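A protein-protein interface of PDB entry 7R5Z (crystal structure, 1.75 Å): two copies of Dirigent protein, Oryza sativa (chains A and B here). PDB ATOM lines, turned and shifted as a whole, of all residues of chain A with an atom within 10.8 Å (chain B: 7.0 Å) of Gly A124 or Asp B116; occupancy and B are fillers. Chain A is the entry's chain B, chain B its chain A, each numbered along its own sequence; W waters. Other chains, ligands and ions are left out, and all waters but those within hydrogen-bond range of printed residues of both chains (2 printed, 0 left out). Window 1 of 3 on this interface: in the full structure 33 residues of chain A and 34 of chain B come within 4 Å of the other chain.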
ATOM      1  N   ASN A  21     -11.560  -6.770  32.926  1.00  0.00           N
ATOM      2  CA  ASN A  21     -12.465  -5.869  32.214  1.00  0.00           C
ATOM      3  C   ASN A  21     -13.347  -6.711  31.302  1.00  0.00           C
ATOM      4  O   ASN A  21     -12.874  -7.216  30.280  1.00  0.00           O
ATOM      5  CB  ASN A  21     -11.687  -4.828  31.423  1.00  0.00           C
ATOM      6  CG  ASN A  21     -12.573  -3.725  30.881  1.00  0.00           C
ATOM      7  OD1 ASN A  21     -12.906  -2.777  31.594  1.00  0.00           O
ATOM      8  ND2 ASN A  21     -12.955  -3.836  29.614  1.00  0.00           N
ATOM      9  N   ILE A  23     -15.984  -7.735  28.508  1.00  0.00           N
ATOM     10  CA  ILE A  23     -16.339  -7.232  27.186  1.00  0.00           C
ATOM     11  C   ILE A  23     -17.861  -7.245  27.094  1.00  0.00           C
ATOM     12  O   ILE A  23     -18.476  -8.289  26.870  1.00  0.00           O
ATOM     13  CB  ILE A  23     -15.700  -8.067  26.077  1.00  0.00           C
ATOM     14  CG1 ILE A  23     -14.185  -8.133  26.273  1.00  0.00           C
ATOM     15  CG2 ILE A  23     -16.039  -7.488  24.714  1.00  0.00           C
ATOM     16  CD1 ILE A  23     -13.525  -9.253  25.513  1.00  0.00           C
ATOM     17  N   SER A  92     -11.029 -11.968  11.406  1.00  0.00           N
ATOM     18  CA  SER A  92     -10.944 -10.741  12.181  1.00  0.00           C
ATOM     19  C   SER A  92     -12.316 -10.093  12.210  1.00  0.00           C
ATOM     20  O   SER A  92     -12.918  -9.862  11.158  1.00  0.00           O
ATOM     21  CB  SER A  92      -9.938  -9.743  11.585  1.00  0.00           C
ATOM     22  OG  SER A  92      -8.614 -10.271  11.541  1.00  0.00           O
ATOM     23  N   LEU A  93     -12.782  -9.762  13.408  1.00  0.00           N
ATOM     24  CA  LEU A  93     -13.986  -8.959  13.584  1.00  0.00           C
ATOM     25  C   LEU A  93     -13.540  -7.507  13.696  1.00  0.00           C
ATOM     26  O   LEU A  93     -13.008  -7.092  14.724  1.00  0.00           O
ATOM     27  CB  LEU A  93     -14.751  -9.428  14.819  1.00  0.00           C
ATOM     28  CG  LEU A  93     -16.141  -8.832  15.008  1.00  0.00           C
ATOM     29  CD1 LEU A  93     -16.944  -9.083  13.757  1.00  0.00           C
ATOM     30  CD2 LEU A  93     -16.813  -9.453  16.241  1.00  0.00           C
ATOM     31  N   VAL A  94     -13.737  -6.742  12.621  1.00  0.00           N
ATOM     32  CA  VAL A  94     -13.187  -5.396  12.475  1.00  0.00           C
ATOM     33  C   VAL A  94     -14.307  -4.392  12.696  1.00  0.00           C
ATOM     34  O   VAL A  94     -15.266  -4.347  11.919  1.00  0.00           O
ATOM     35  CB  VAL A  94     -12.563  -5.209  11.087  1.00  0.00           C
ATOM     36  CG1 VAL A  94     -11.810  -3.880  11.002  1.00  0.00           C
ATOM     37  CG2 VAL A  94     -11.674  -6.399  10.770  1.00  0.00           C
ATOM     38  N   PHE A  95     -14.190  -3.581  13.741  1.00  0.00           N
ATOM     39  CA  PHE A  95     -15.251  -2.648  14.086  1.00  0.00           C
ATOM     40  C   PHE A  95     -15.074  -1.325  13.356  1.00  0.00           C
ATOM     41  O   PHE A  95     -13.954  -0.883  13.092  1.00  0.00           O
ATOM     42  CB  PHE A  95     -15.287  -2.419  15.592  1.00  0.00           C
ATOM     43  CG  PHE A  95     -15.729  -3.618  16.355  1.00  0.00           C
ATOM     44  CD1 PHE A  95     -17.073  -3.839  16.591  1.00  0.00           C
ATOM     45  CD2 PHE A  95     -14.804  -4.550  16.807  1.00  0.00           C
ATOM     46  CE1 PHE A  95     -17.498  -4.961  17.293  1.00  0.00           C
ATOM     47  CE2 PHE A  95     -15.217  -5.663  17.500  1.00  0.00           C
ATOM     48  CZ  PHE A  95     -16.571  -5.875  17.746  1.00  0.00           C
ATOM     49  N   ASP A  97     -17.160   1.851  14.038  1.00  0.00           N
ATOM     50  CA  ASP A  97     -17.468   3.105  14.713  1.00  0.00           C
ATOM     51  C   ASP A  97     -16.214   3.755  15.287  1.00  0.00           C
ATOM     52  O   ASP A  97     -15.239   3.083  15.631  1.00  0.00           O
ATOM     53  CB  ASP A  97     -18.478   2.871  15.836  1.00  0.00           C
ATOM     54  CG  ASP A  97     -19.849   2.494  15.316  1.00  0.00           C
ATOM     55  OD1 ASP A  97     -20.005   2.363  14.084  1.00  0.00           O
ATOM     56  OD2 ASP A  97     -20.772   2.333  16.142  1.00  0.00           O
ATOM     57  N   ARG A  99     -13.916   5.577  18.105  1.00  0.00           N
ATOM     58  CA  ARG A  99     -13.501   5.027  19.396  1.00  0.00           C
ATOM     59  C   ARG A  99     -13.213   3.536  19.267  1.00  0.00           C
ATOM     60  O   ARG A  99     -12.153   3.067  19.693  1.00  0.00           O
ATOM     61  CB  ARG A  99     -14.541   5.284  20.492  1.00  0.00           C
ATOM     62  N   LEU A 100     -14.143   2.782  18.684  1.00  0.00           N
ATOM     63  CA  LEU A 100     -13.894   1.379  18.376  1.00  0.00           C
ATOM     64  C   LEU A 100     -13.179   1.183  17.048  1.00  0.00           C
ATOM     65  O   LEU A 100     -12.933   0.033  16.664  1.00  0.00           O
ATOM     66  CB  LEU A 100     -15.207   0.593  18.369  1.00  0.00           C
ATOM     67  CG  LEU A 100     -15.630   0.044  19.730  1.00  0.00           C
ATOM     68  CD1 LEU A 100     -16.876  -0.821  19.603  1.00  0.00           C
ATOM     69  CD2 LEU A 100     -14.483  -0.737  20.350  1.00  0.00           C
ATOM     70  N   LYS A 101     -12.845   2.265  16.346  1.00  0.00           N
ATOM     71  CA  LYS A 101     -12.159   2.149  15.069  1.00  0.00           C
ATOM     72  C   LYS A 101     -10.801   1.486  15.254  1.00  0.00           C
ATOM     73  O   LYS A 101     -10.106   1.716  16.247  1.00  0.00           O
ATOM     74  CB  LYS A 101     -11.990   3.526  14.428  1.00  0.00           C
ATOM     75  N   GLY A 102     -10.435   0.643  14.292  1.00  0.00           N
ATOM     76  CA  GLY A 102      -9.161  -0.044  14.332  1.00  0.00           C
ATOM     77  C   GLY A 102      -9.179  -1.301  15.174  1.00  0.00           C
ATOM     78  O   GLY A 102      -8.484  -2.272  14.859  1.00  0.00           O
ATOM     79  N   SER A 103      -9.980  -1.296  16.240  1.00  0.00           N
ATOM     80  CA  SER A 103      -9.990  -2.400  17.187  1.00  0.00           C
ATOM     81  C   SER A 103     -10.638  -3.630  16.571  1.00  0.00           C
ATOM     82  O   SER A 103     -11.588  -3.533  15.789  1.00  0.00           O
ATOM     83  CB  SER A 103     -10.730  -2.003  18.464  1.00  0.00           C
ATOM     84  OG  SER A 103      -9.946  -1.143  19.270  1.00  0.00           O
ATOM     85  N   THR A 104     -10.111  -4.796  16.921  1.00  0.00           N
ATOM     86  CA  THR A 104     -10.594  -6.051  16.363  1.00  0.00           C
ATOM     87  C   THR A 104     -10.701  -7.094  17.462  1.00  0.00           C
ATOM     88  O   THR A 104      -9.996  -7.024  18.471  1.00  0.00           O
ATOM     89  CB  THR A 104      -9.679  -6.613  15.263  1.00  0.00           C
ATOM     90  OG1 THR A 104      -8.475  -7.127  15.849  1.00  0.00           O
ATOM     91  CG2 THR A 104      -9.334  -5.550  14.236  1.00  0.00           C
ATOM     92  N   LEU A 105     -11.594  -8.060  17.249  1.00  0.00           N
ATOM     93  CA  LEU A 105     -11.594  -9.323  17.969  1.00  0.00           C
ATOM     94  C   LEU A 105     -11.174 -10.425  17.014  1.00  0.00           C
ATOM     95  O   LEU A 105     -11.580 -10.439  15.850  1.00  0.00           O
ATOM     96  CB  LEU A 105     -12.974  -9.651  18.551  1.00  0.00           C
ATOM     97  CG  LEU A 105     -13.437  -8.750  19.686  1.00  0.00           C
ATOM     98  CD1 LEU A 105     -14.927  -8.914  19.911  1.00  0.00           C
ATOM     99  CD2 LEU A 105     -12.669  -9.115  20.934  1.00  0.00           C
ATOM    100  N   GLN A 106     -10.322 -11.320  17.487  1.00  0.00           N
ATOM    101  CA  GLN A 106      -9.865 -12.435  16.677  1.00  0.00           C
ATOM    102  C   GLN A 106     -10.709 -13.638  17.060  1.00  0.00           C
ATOM    103  O   GLN A 106     -10.876 -13.918  18.251  1.00  0.00           O
ATOM    104  CB  GLN A 106      -8.377 -12.694  16.892  1.00  0.00           C
ATOM    105  CG  GLN A 106      -7.531 -11.486  16.434  1.00  0.00           C
ATOM    106  CD  GLN A 106      -7.803 -11.117  14.971  1.00  0.00           C
ATOM    107  OE1 GLN A 106      -7.789 -11.981  14.099  1.00  0.00           O
ATOM    108  NE2 GLN A 106      -8.071  -9.843  14.715  1.00  0.00           N
ATOM    109  N   GLY A 121      -8.218 -13.591  20.826  1.00  0.00           N
ATOM    110  CA  GLY A 121      -7.347 -12.441  20.971  1.00  0.00           C
ATOM    111  C   GLY A 121      -8.068 -11.194  20.515  1.00  0.00           C
ATOM    112  O   GLY A 121      -9.255 -11.220  20.177  1.00  0.00           O
ATOM    113  N   GLY A 122      -7.328 -10.091  20.514  1.00  0.00           N
ATOM    114  CA  GLY A 122      -7.890  -8.847  20.020  1.00  0.00           C
ATOM    115  C   GLY A 122      -6.830  -7.778  19.982  1.00  0.00           C
ATOM    116  O   GLY A 122      -5.677  -8.010  20.358  1.00  0.00           O
ATOM    117  N   THR A 123      -7.240  -6.599  19.494  1.00  0.00           N
ATOM    118  CA  THR A 123      -6.351  -5.454  19.307  1.00  0.00           C
ATOM    119  C   THR A 123      -7.092  -4.183  19.679  1.00  0.00           C
ATOM    120  O   THR A 123      -8.319  -4.168  19.798  1.00  0.00           O
ATOM    121  CB  THR A 123      -5.851  -5.316  17.858  1.00  0.00           C
ATOM    122  OG1 THR A 123      -6.971  -5.223  16.968  1.00  0.00           O
ATOM    123  CG2 THR A 123      -4.974  -6.475  17.463  1.00  0.00           C
ATOM    124  N   GLY A 124      -6.332  -3.097  19.824  1.00  0.00           N
ATOM    125  CA  GLY A 124      -6.940  -1.836  20.197  1.00  0.00           C
ATOM    126  C   GLY A 124      -7.530  -1.963  21.582  1.00  0.00           C
ATOM    127  O   GLY A 124      -6.884  -2.442  22.519  1.00  0.00           O
ATOM    128  N   GLN A 125      -8.786  -1.561  21.718  1.00  0.00           N
ATOM    129  CA  GLN A 125      -9.439  -1.661  23.014  1.00  0.00           C
ATOM    130  C   GLN A 125      -9.652  -3.105  23.462  1.00  0.00           C
ATOM    131  O   GLN A 125      -9.899  -3.329  24.651  1.00  0.00           O
ATOM    132  CB  GLN A 125     -10.760  -0.895  22.970  1.00  0.00           C
ATOM    133  CG  GLN A 125     -10.558   0.565  22.578  1.00  0.00           C
ATOM    134  CD  GLN A 125     -11.846   1.354  22.540  1.00  0.00           C
ATOM    135  OE1 GLN A 125     -12.926   0.809  22.760  1.00  0.00           O
ATOM    136  NE2 GLN A 125     -11.739   2.646  22.260  1.00  0.00           N
ATOM    137  N   PHE A 126      -9.515  -4.087  22.562  1.00  0.00           N
ATOM    138  CA  PHE A 126      -9.708  -5.493  22.893  1.00  0.00           C
ATOM    139  C   PHE A 126      -8.395  -6.258  22.976  1.00  0.00           C
ATOM    140  O   PHE A 126      -8.378  -7.474  22.776  1.00  0.00           O
ATOM    141  CB  PHE A 126     -10.650  -6.133  21.877  1.00  0.00           C
ATOM    142  CG  PHE A 126     -11.973  -5.443  21.799  1.00  0.00           C
ATOM    143  CD1 PHE A 126     -12.683  -5.173  22.955  1.00  0.00           C
ATOM    144  CD2 PHE A 126     -12.488  -5.026  20.587  1.00  0.00           C
ATOM    145  CE1 PHE A 126     -13.896  -4.511  22.903  1.00  0.00           C
ATOM    146  CE2 PHE A 126     -13.703  -4.367  20.527  1.00  0.00           C
ATOM    147  CZ  PHE A 126     -14.405  -4.110  21.684  1.00  0.00           C
ATOM    148  N   ALA A 127      -7.290  -5.565  23.246  1.00  0.00           N
ATOM    149  CA  ALA A 127      -6.013  -6.244  23.404  1.00  0.00           C
ATOM    150  C   ALA A 127      -6.119  -7.314  24.483  1.00  0.00           C
ATOM    151  O   ALA A 127      -6.624  -7.063  25.586  1.00  0.00           O
ATOM    152  CB  ALA A 127      -4.916  -5.236  23.745  1.00  0.00           C
ATOM    153  N   MET A 128      -5.690  -8.530  24.130  1.00  0.00           N
ATOM    154  CA  MET A 128      -5.674  -9.696  25.007  1.00  0.00           C
ATOM    155  C   MET A 128      -7.066 -10.258  25.288  1.00  0.00           C
ATOM    156  O   MET A 128      -7.240 -11.005  26.253  1.00  0.00           O
ATOM    157  CB  MET A 128      -4.948  -9.386  26.324  1.00  0.00           C
ATOM    158  CG  MET A 128      -3.476  -9.003  26.128  1.00  0.00           C
ATOM    159  SD  MET A 128      -2.656  -8.635  27.695  1.00  0.00           S
ATOM    160  CE  MET A 128      -3.429  -7.073  28.104  1.00  0.00           C
ATOM    161  N   ALA A 129      -8.058  -9.927  24.459  1.00  0.00           N
ATOM    162  CA  ALA A 129      -9.413 -10.435  24.648  1.00  0.00           C
ATOM    163  C   ALA A 129      -9.442 -11.962  24.697  1.00  0.00           C
ATOM    164  O   ALA A 129      -8.709 -12.637  23.970  1.00  0.00           O
ATOM    165  CB  ALA A 129     -10.322  -9.942  23.523  1.00  0.00           C
ATOM    166  N   PHE A 154     -13.568 -11.311  28.277  1.00  0.00           N
ATOM    167  CA  PHE A 154     -12.880 -10.382  29.157  1.00  0.00           C
ATOM    168  C   PHE A 154     -11.606  -9.901  28.489  1.00  0.00           C
ATOM    169  O   PHE A 154     -11.013 -10.598  27.662  1.00  0.00           O
ATOM    170  CB  PHE A 154     -12.509 -11.024  30.501  1.00  0.00           C
ATOM    171  CG  PHE A 154     -13.663 -11.650  31.205  1.00  0.00           C
ATOM    172  CD1 PHE A 154     -14.017 -12.964  30.946  1.00  0.00           C
ATOM    173  CD2 PHE A 154     -14.404 -10.926  32.126  1.00  0.00           C
ATOM    174  CE1 PHE A 154     -15.092 -13.541  31.591  1.00  0.00           C
ATOM    175  CE2 PHE A 154     -15.481 -11.501  32.778  1.00  0.00           C
ATOM    176  CZ  PHE A 154     -15.821 -12.804  32.513  1.00  0.00           C
ATOM    177  N   CYS A 155     -11.197  -8.696  28.862  1.00  0.00           N
ATOM    178  CA  CYS A 155      -9.847  -8.227  28.616  1.00  0.00           C
ATOM    179  C   CYS A 155      -9.135  -8.128  29.952  1.00  0.00           C
ATOM    180  O   CYS A 155      -9.603  -7.400  30.836  1.00  0.00           O
ATOM    181  CB  CYS A 155      -9.852  -6.877  27.910  1.00  0.00           C
ATOM    182  SG  CYS A 155     -10.501  -6.968  26.240  1.00  0.00           S
ATOM    183  N   PRO A 156      -8.042  -8.848  30.159  1.00  0.00           N
ATOM    184  CA  PRO A 156      -7.364  -8.795  31.452  1.00  0.00           C
ATOM    185  C   PRO A 156      -6.570  -7.510  31.617  1.00  0.00           C
ATOM    186  O   PRO A 156      -6.040  -6.942  30.660  1.00  0.00           O
ATOM    187  CB  PRO A 156      -6.442 -10.016  31.407  1.00  0.00           C
ATOM    188  CG  PRO A 156      -6.120 -10.166  29.963  1.00  0.00           C
ATOM    189  CD  PRO A 156      -7.386  -9.785  29.230  1.00  0.00           C
ATOM    190  N   MET B 108      -2.331 -13.397  14.851  1.00  0.00           N
ATOM    191  CA  MET B 108      -3.548 -13.396  14.064  1.00  0.00           C
ATOM    192  C   MET B 108      -4.082 -11.976  13.968  1.00  0.00           C
ATOM    193  O   MET B 108      -4.100 -11.251  14.964  1.00  0.00           O
ATOM    194  CB  MET B 108      -4.570 -14.324  14.721  1.00  0.00           C
ATOM    195  CG  MET B 108      -5.947 -14.297  14.148  1.00  0.00           C
ATOM    196  SD  MET B 108      -6.849 -15.624  14.957  1.00  0.00           S
ATOM    197  CE  MET B 108      -5.665 -16.880  14.624  1.00  0.00           C
ATOM    198  N   GLY B 109      -4.508 -11.575  12.781  1.00  0.00           N
ATOM    199  CA  GLY B 109      -5.188 -10.306  12.667  1.00  0.00           C
ATOM    200  C   GLY B 109      -5.073  -9.670  11.299  1.00  0.00           C
ATOM    201  O   GLY B 109      -4.549 -10.241  10.351  1.00  0.00           O
ATOM    202  N   LEU B 110      -5.555  -8.441  11.253  1.00  0.00           N
ATOM    203  CA  LEU B 110      -5.795  -7.712  10.019  1.00  0.00           C
ATOM    204  C   LEU B 110      -4.637  -6.771   9.702  1.00  0.00           C
ATOM    205  O   LEU B 110      -4.070  -6.145  10.608  1.00  0.00           O
ATOM    206  CB  LEU B 110      -7.095  -6.913  10.135  1.00  0.00           C
ATOM    207  CG  LEU B 110      -7.741  -6.635   8.773  1.00  0.00           C
ATOM    208  CD1 LEU B 110      -8.351  -7.913   8.205  1.00  0.00           C
ATOM    209  CD2 LEU B 110      -8.770  -5.530   8.869  1.00  0.00           C
ATOM    210  N   ILE B 111      -4.316  -6.681   8.407  1.00  0.00           N
ATOM    211  CA  ILE B 111      -3.399  -5.716   7.782  1.00  0.00           C
ATOM    212  C   ILE B 111      -1.951  -6.171   7.956  1.00  0.00           C
ATOM    213  O   ILE B 111      -1.551  -6.660   9.022  1.00  0.00           O
ATOM    214  CB  ILE B 111      -3.597  -4.287   8.319  1.00  0.00           C
ATOM    215  CG1 ILE B 111      -5.068  -3.888   8.264  1.00  0.00           C
ATOM    216  CG2 ILE B 111      -2.834  -3.280   7.439  1.00  0.00           C
ATOM    217  CD1 ILE B 111      -5.385  -2.623   9.018  1.00  0.00           C
ATOM    218  N   GLU B 114       0.564  -2.091   8.686  1.00  0.00           N
ATOM    219  CA  GLU B 114       0.159  -1.037   9.604  1.00  0.00           C
ATOM    220  C   GLU B 114      -0.844  -1.645  10.566  1.00  0.00           C
ATOM    221  O   GLU B 114      -1.282  -2.776  10.386  1.00  0.00           O
ATOM    222  CB  GLU B 114      -0.451   0.166   8.874  1.00  0.00           C
ATOM    223  CG  GLU B 114       0.532   0.962   7.995  1.00  0.00           C
ATOM    224  CD  GLU B 114       1.622   1.683   8.798  1.00  0.00           C
ATOM    225  OE1 GLU B 114       1.561   1.685  10.048  1.00  0.00           O
ATOM    226  OE2 GLU B 114       2.542   2.257   8.173  1.00  0.00           O
ATOM    227  N   GLY B 115      -1.221  -0.885  11.583  1.00  0.00           N
ATOM    228  CA  GLY B 115      -2.178  -1.406  12.541  1.00  0.00           C
ATOM    229  C   GLY B 115      -1.563  -2.420  13.496  1.00  0.00           C
ATOM    230  O   GLY B 115      -0.372  -2.382  13.806  1.00  0.00           O
ATOM    231  N   ASP B 116      -2.405  -3.331  13.989  1.00  0.00           N
ATOM    232  CA  ASP B 116      -2.007  -4.241  15.053  1.00  0.00           C
ATOM    233  C   ASP B 116      -2.404  -5.666  14.689  1.00  0.00           C
ATOM    234  O   ASP B 116      -3.332  -5.886  13.906  1.00  0.00           O
ATOM    235  CB  ASP B 116      -2.661  -3.874  16.407  1.00  0.00           C
ATOM    236  CG  ASP B 116      -2.484  -2.417  16.780  1.00  0.00           C
ATOM    237  OD1 ASP B 116      -1.536  -1.757  16.285  1.00  0.00           O
ATOM    238  OD2 ASP B 116      -3.298  -1.923  17.590  1.00  0.00           O
ATOM    239  N   TRP B 117      -1.653  -6.624  15.228  1.00  0.00           N
ATOM    240  CA  TRP B 117      -2.006  -8.035  15.236  1.00  0.00           C
ATOM    241  C   TRP B 117      -2.210  -8.472  16.676  1.00  0.00           C
ATOM    242  O   TRP B 117      -1.610  -7.901  17.587  1.00  0.00           O
ATOM    243  CB  TRP B 117      -0.904  -8.905  14.652  1.00  0.00           C
ATOM    244  CG  TRP B 117      -0.762  -8.861  13.172  1.00  0.00           C
ATOM    245  CD1 TRP B 117      -1.760  -8.827  12.257  1.00  0.00           C
ATOM    246  CD2 TRP B 117       0.461  -8.892  12.445  1.00  0.00           C
ATOM    247  NE1 TRP B 117      -1.237  -8.822  10.991  1.00  0.00           N
ATOM    248  CE2 TRP B 117       0.129  -8.882  11.075  1.00  0.00           C
ATOM    249  CE3 TRP B 117       1.809  -8.940  12.813  1.00  0.00           C
ATOM    250  CZ2 TRP B 117       1.092  -8.889  10.075  1.00  0.00           C
ATOM    251  CZ3 TRP B 117       2.780  -8.939  11.807  1.00  0.00           C
ATOM    252  CH2 TRP B 117       2.415  -8.923  10.457  1.00  0.00           C
ATOM    253  N   ALA B 118      -3.035  -9.503  16.868  1.00  0.00           N
ATOM    254  CA  ALA B 118      -3.186 -10.123  18.175  1.00  0.00           C
ATOM    255  C   ALA B 118      -2.146 -11.213  18.369  1.00  0.00           C
ATOM    256  O   ALA B 118      -1.873 -12.000  17.459  1.00  0.00           O
ATOM    257  CB  ALA B 118      -4.582 -10.737  18.345  1.00  0.00           C
ATOM    258  N   VAL B 132      -0.326  -8.135  21.847  1.00  0.00           N
ATOM    259  CA  VAL B 132      -0.503  -7.544  20.529  1.00  0.00           C
ATOM    260  C   VAL B 132       0.864  -7.341  19.901  1.00  0.00           C
ATOM    261  O   VAL B 132       1.887  -7.241  20.586  1.00  0.00           O
ATOM    262  CB  VAL B 132      -1.242  -6.190  20.574  1.00  0.00           C
ATOM    263  CG1 VAL B 132      -2.648  -6.359  21.120  1.00  0.00           C
ATOM    264  CG2 VAL B 132      -0.431  -5.174  21.415  1.00  0.00           C
ATOM    265  N   ILE B 133       0.862  -7.234  18.581  1.00  0.00           N
ATOM    266  CA  ILE B 133       2.034  -6.805  17.832  1.00  0.00           C
ATOM    267  C   ILE B 133       1.645  -5.539  17.082  1.00  0.00           C
ATOM    268  O   ILE B 133       0.626  -5.523  16.383  1.00  0.00           O
ATOM    269  CB  ILE B 133       2.518  -7.890  16.851  1.00  0.00           C
ATOM    270  CG1 ILE B 133       2.931  -9.134  17.631  1.00  0.00           C
ATOM    271  CG2 ILE B 133       3.705  -7.366  16.026  1.00  0.00           C
ATOM    272  CD1 ILE B 133       3.520 -10.218  16.792  1.00  0.00           C
ATOM    273  N   LEU B 134       2.433  -4.477  17.246  1.00  0.00           N
ATOM    274  CA  LEU B 134       2.196  -3.231  16.527  1.00  0.00           C
ATOM    275  C   LEU B 134       3.090  -3.167  15.293  1.00  0.00           C
ATOM    276  O   LEU B 134       4.287  -3.464  15.379  1.00  0.00           O
ATOM    277  CB  LEU B 134       2.445  -2.024  17.427  1.00  0.00           C
ATOM    278  CG  LEU B 134       1.863  -2.086  18.849  1.00  0.00           C
ATOM    279  CD1 LEU B 134       2.178  -0.787  19.563  1.00  0.00           C
ATOM    280  CD2 LEU B 134       0.368  -2.344  18.821  1.00  0.00           C
ATOM    281  N   LYS B 135       2.507  -2.773  14.151  1.00  0.00           N
ATOM    282  CA  LYS B 135       3.205  -2.690  12.871  1.00  0.00           C
ATOM    283  C   LYS B 135       3.357  -1.237  12.447  1.00  0.00           C
ATOM    284  O   LYS B 135       2.414  -0.449  12.550  1.00  0.00           O
ATOM    285  CB  LYS B 135       2.451  -3.428  11.752  1.00  0.00           C
ATOM    286  CG  LYS B 135       2.385  -4.945  11.876  1.00  0.00           C
ATOM    287  CD  LYS B 135       1.127  -5.475  11.164  1.00  0.00           C
ATOM    288  CE  LYS B 135      -0.059  -5.457  12.144  1.00  0.00           C
ATOM    289  NZ  LYS B 135      -1.369  -5.384  11.438  1.00  0.00           N
HETATM  290  O   HOH W   1      -3.660  -3.129  19.883  1.00  0.00           O
HETATM  291  O   HOH W   2      -6.082  -7.118  13.729  1.00  0.00           O
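Hydrophobic or aromatic side chains of chain A that line the printed part of chain B: Val A94 and Ala A127. Of the 13 printed residues of chain B, 7 touch a printed residue of chain A. Hydrophobic or aromatic side chains of chain B that line the printed part of chain A: Met B108, Leu B110, Ala B118 and Val B132. Along chain B the printed residues that touch a printed residue of chain A span positions 108 to 132. Among the printed residues, no Asp or Glu carboxylate lies within 4 Å of a Lys or Arg side-chain nitrogen of the other chain.
Printed residues of chain B within 4 Å of Val A94: Leu B110. Of the printed residues of chain B, Thr A123 touches Asp B116, Trp B117 and Ala B118. Of chain B, only Asp B116 (3.9 Å) comes within 4 Å of Gly A124. Gly B109 touches two residues of chain A. No residue of chain A comes within 4 Å of Ile B111. No residue of chain A comes within 4 Å of Gly B115. Asp B116 touches just these residues of chain A: Thr A123 and Gly A124. Printed residues of chain A within 4 Å of Trp B117: Thr A123 (3.5 Å). Of the printed residues of chain A, Val B132 touches Gly A122 and Ala A127. No residue of chain A comes within 4 Å of Leu B134. Lys B135 touches none of the printed residues of chain A. The nearest residue of chain A that does not touch Asp B116 is Thr A104 (5.6 Å). The nearest printed residue of chain B that does not touch Val A94 is Ile B111 (6.8 Å).
Ser A92 touches Leu B110. Met B108 touches Gln A106. Gly B109 touches Gln A106 (CA to OE1, 3.4 Å). Gly A122 touches Ala B118 (N to CB, 3.6 Å). Gly A122 touches Val B132 (O to CG1, 3.5 Å). CG2 of Thr A123 touches CB of Asp B116, 3.6 Å away. Thr A123 touches Trp B117. CG2 of Thr A123 touches N of Ala B118, at 3.6 Å. Asp B116 touches Gly A124. CB of Ala A127 touches CG1 of Val B132, at 3.6 Å.
Water W1 lies within hydrogen-bond range of the side-chain carboxylate (OD2) of Asp B116 (2.6 Å) and the backbone NH (N) of Gly A124 (2.7 Å). Water W2 lies within hydrogen-bond range of the backbone NH of Leu B110, the backbone carbonyl oxygen of Asp B116 and the side-chain hydroxyl of Thr A104.
No position is printed for both chains.
The backbone carbonyl oxygen (O) of Thr A123 is in hydrogen-bond range of the side-chain hydroxyl (OG) of Ser A103 (3.5 Å). The backbone carbonyl oxygen (O) of Met B108 lies within hydrogen-bond range of the backbone NH (N) of Ala B118, 2.8 Å away. The side-chain amide oxygen (OE1) of Gln A106 is in hydrogen-bond range of the side-chain hydroxyl (OG) of Ser A92. The backbone carbonyl oxygen (O) of Ile B111 lies within hydrogen-bond range of the indole nitrogen (NE1) of Trp B117 (2.9 Å). The backbone carbonyl oxygen of Trp B117 sits at hydrogen-bond distance from the backbone NH of Ile B133 (2.7 Å). The backbone carbonyl oxygen (O) of Leu B110 lies within hydrogen-bond range of the side-chain amino group (NZ) of Lys B135.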
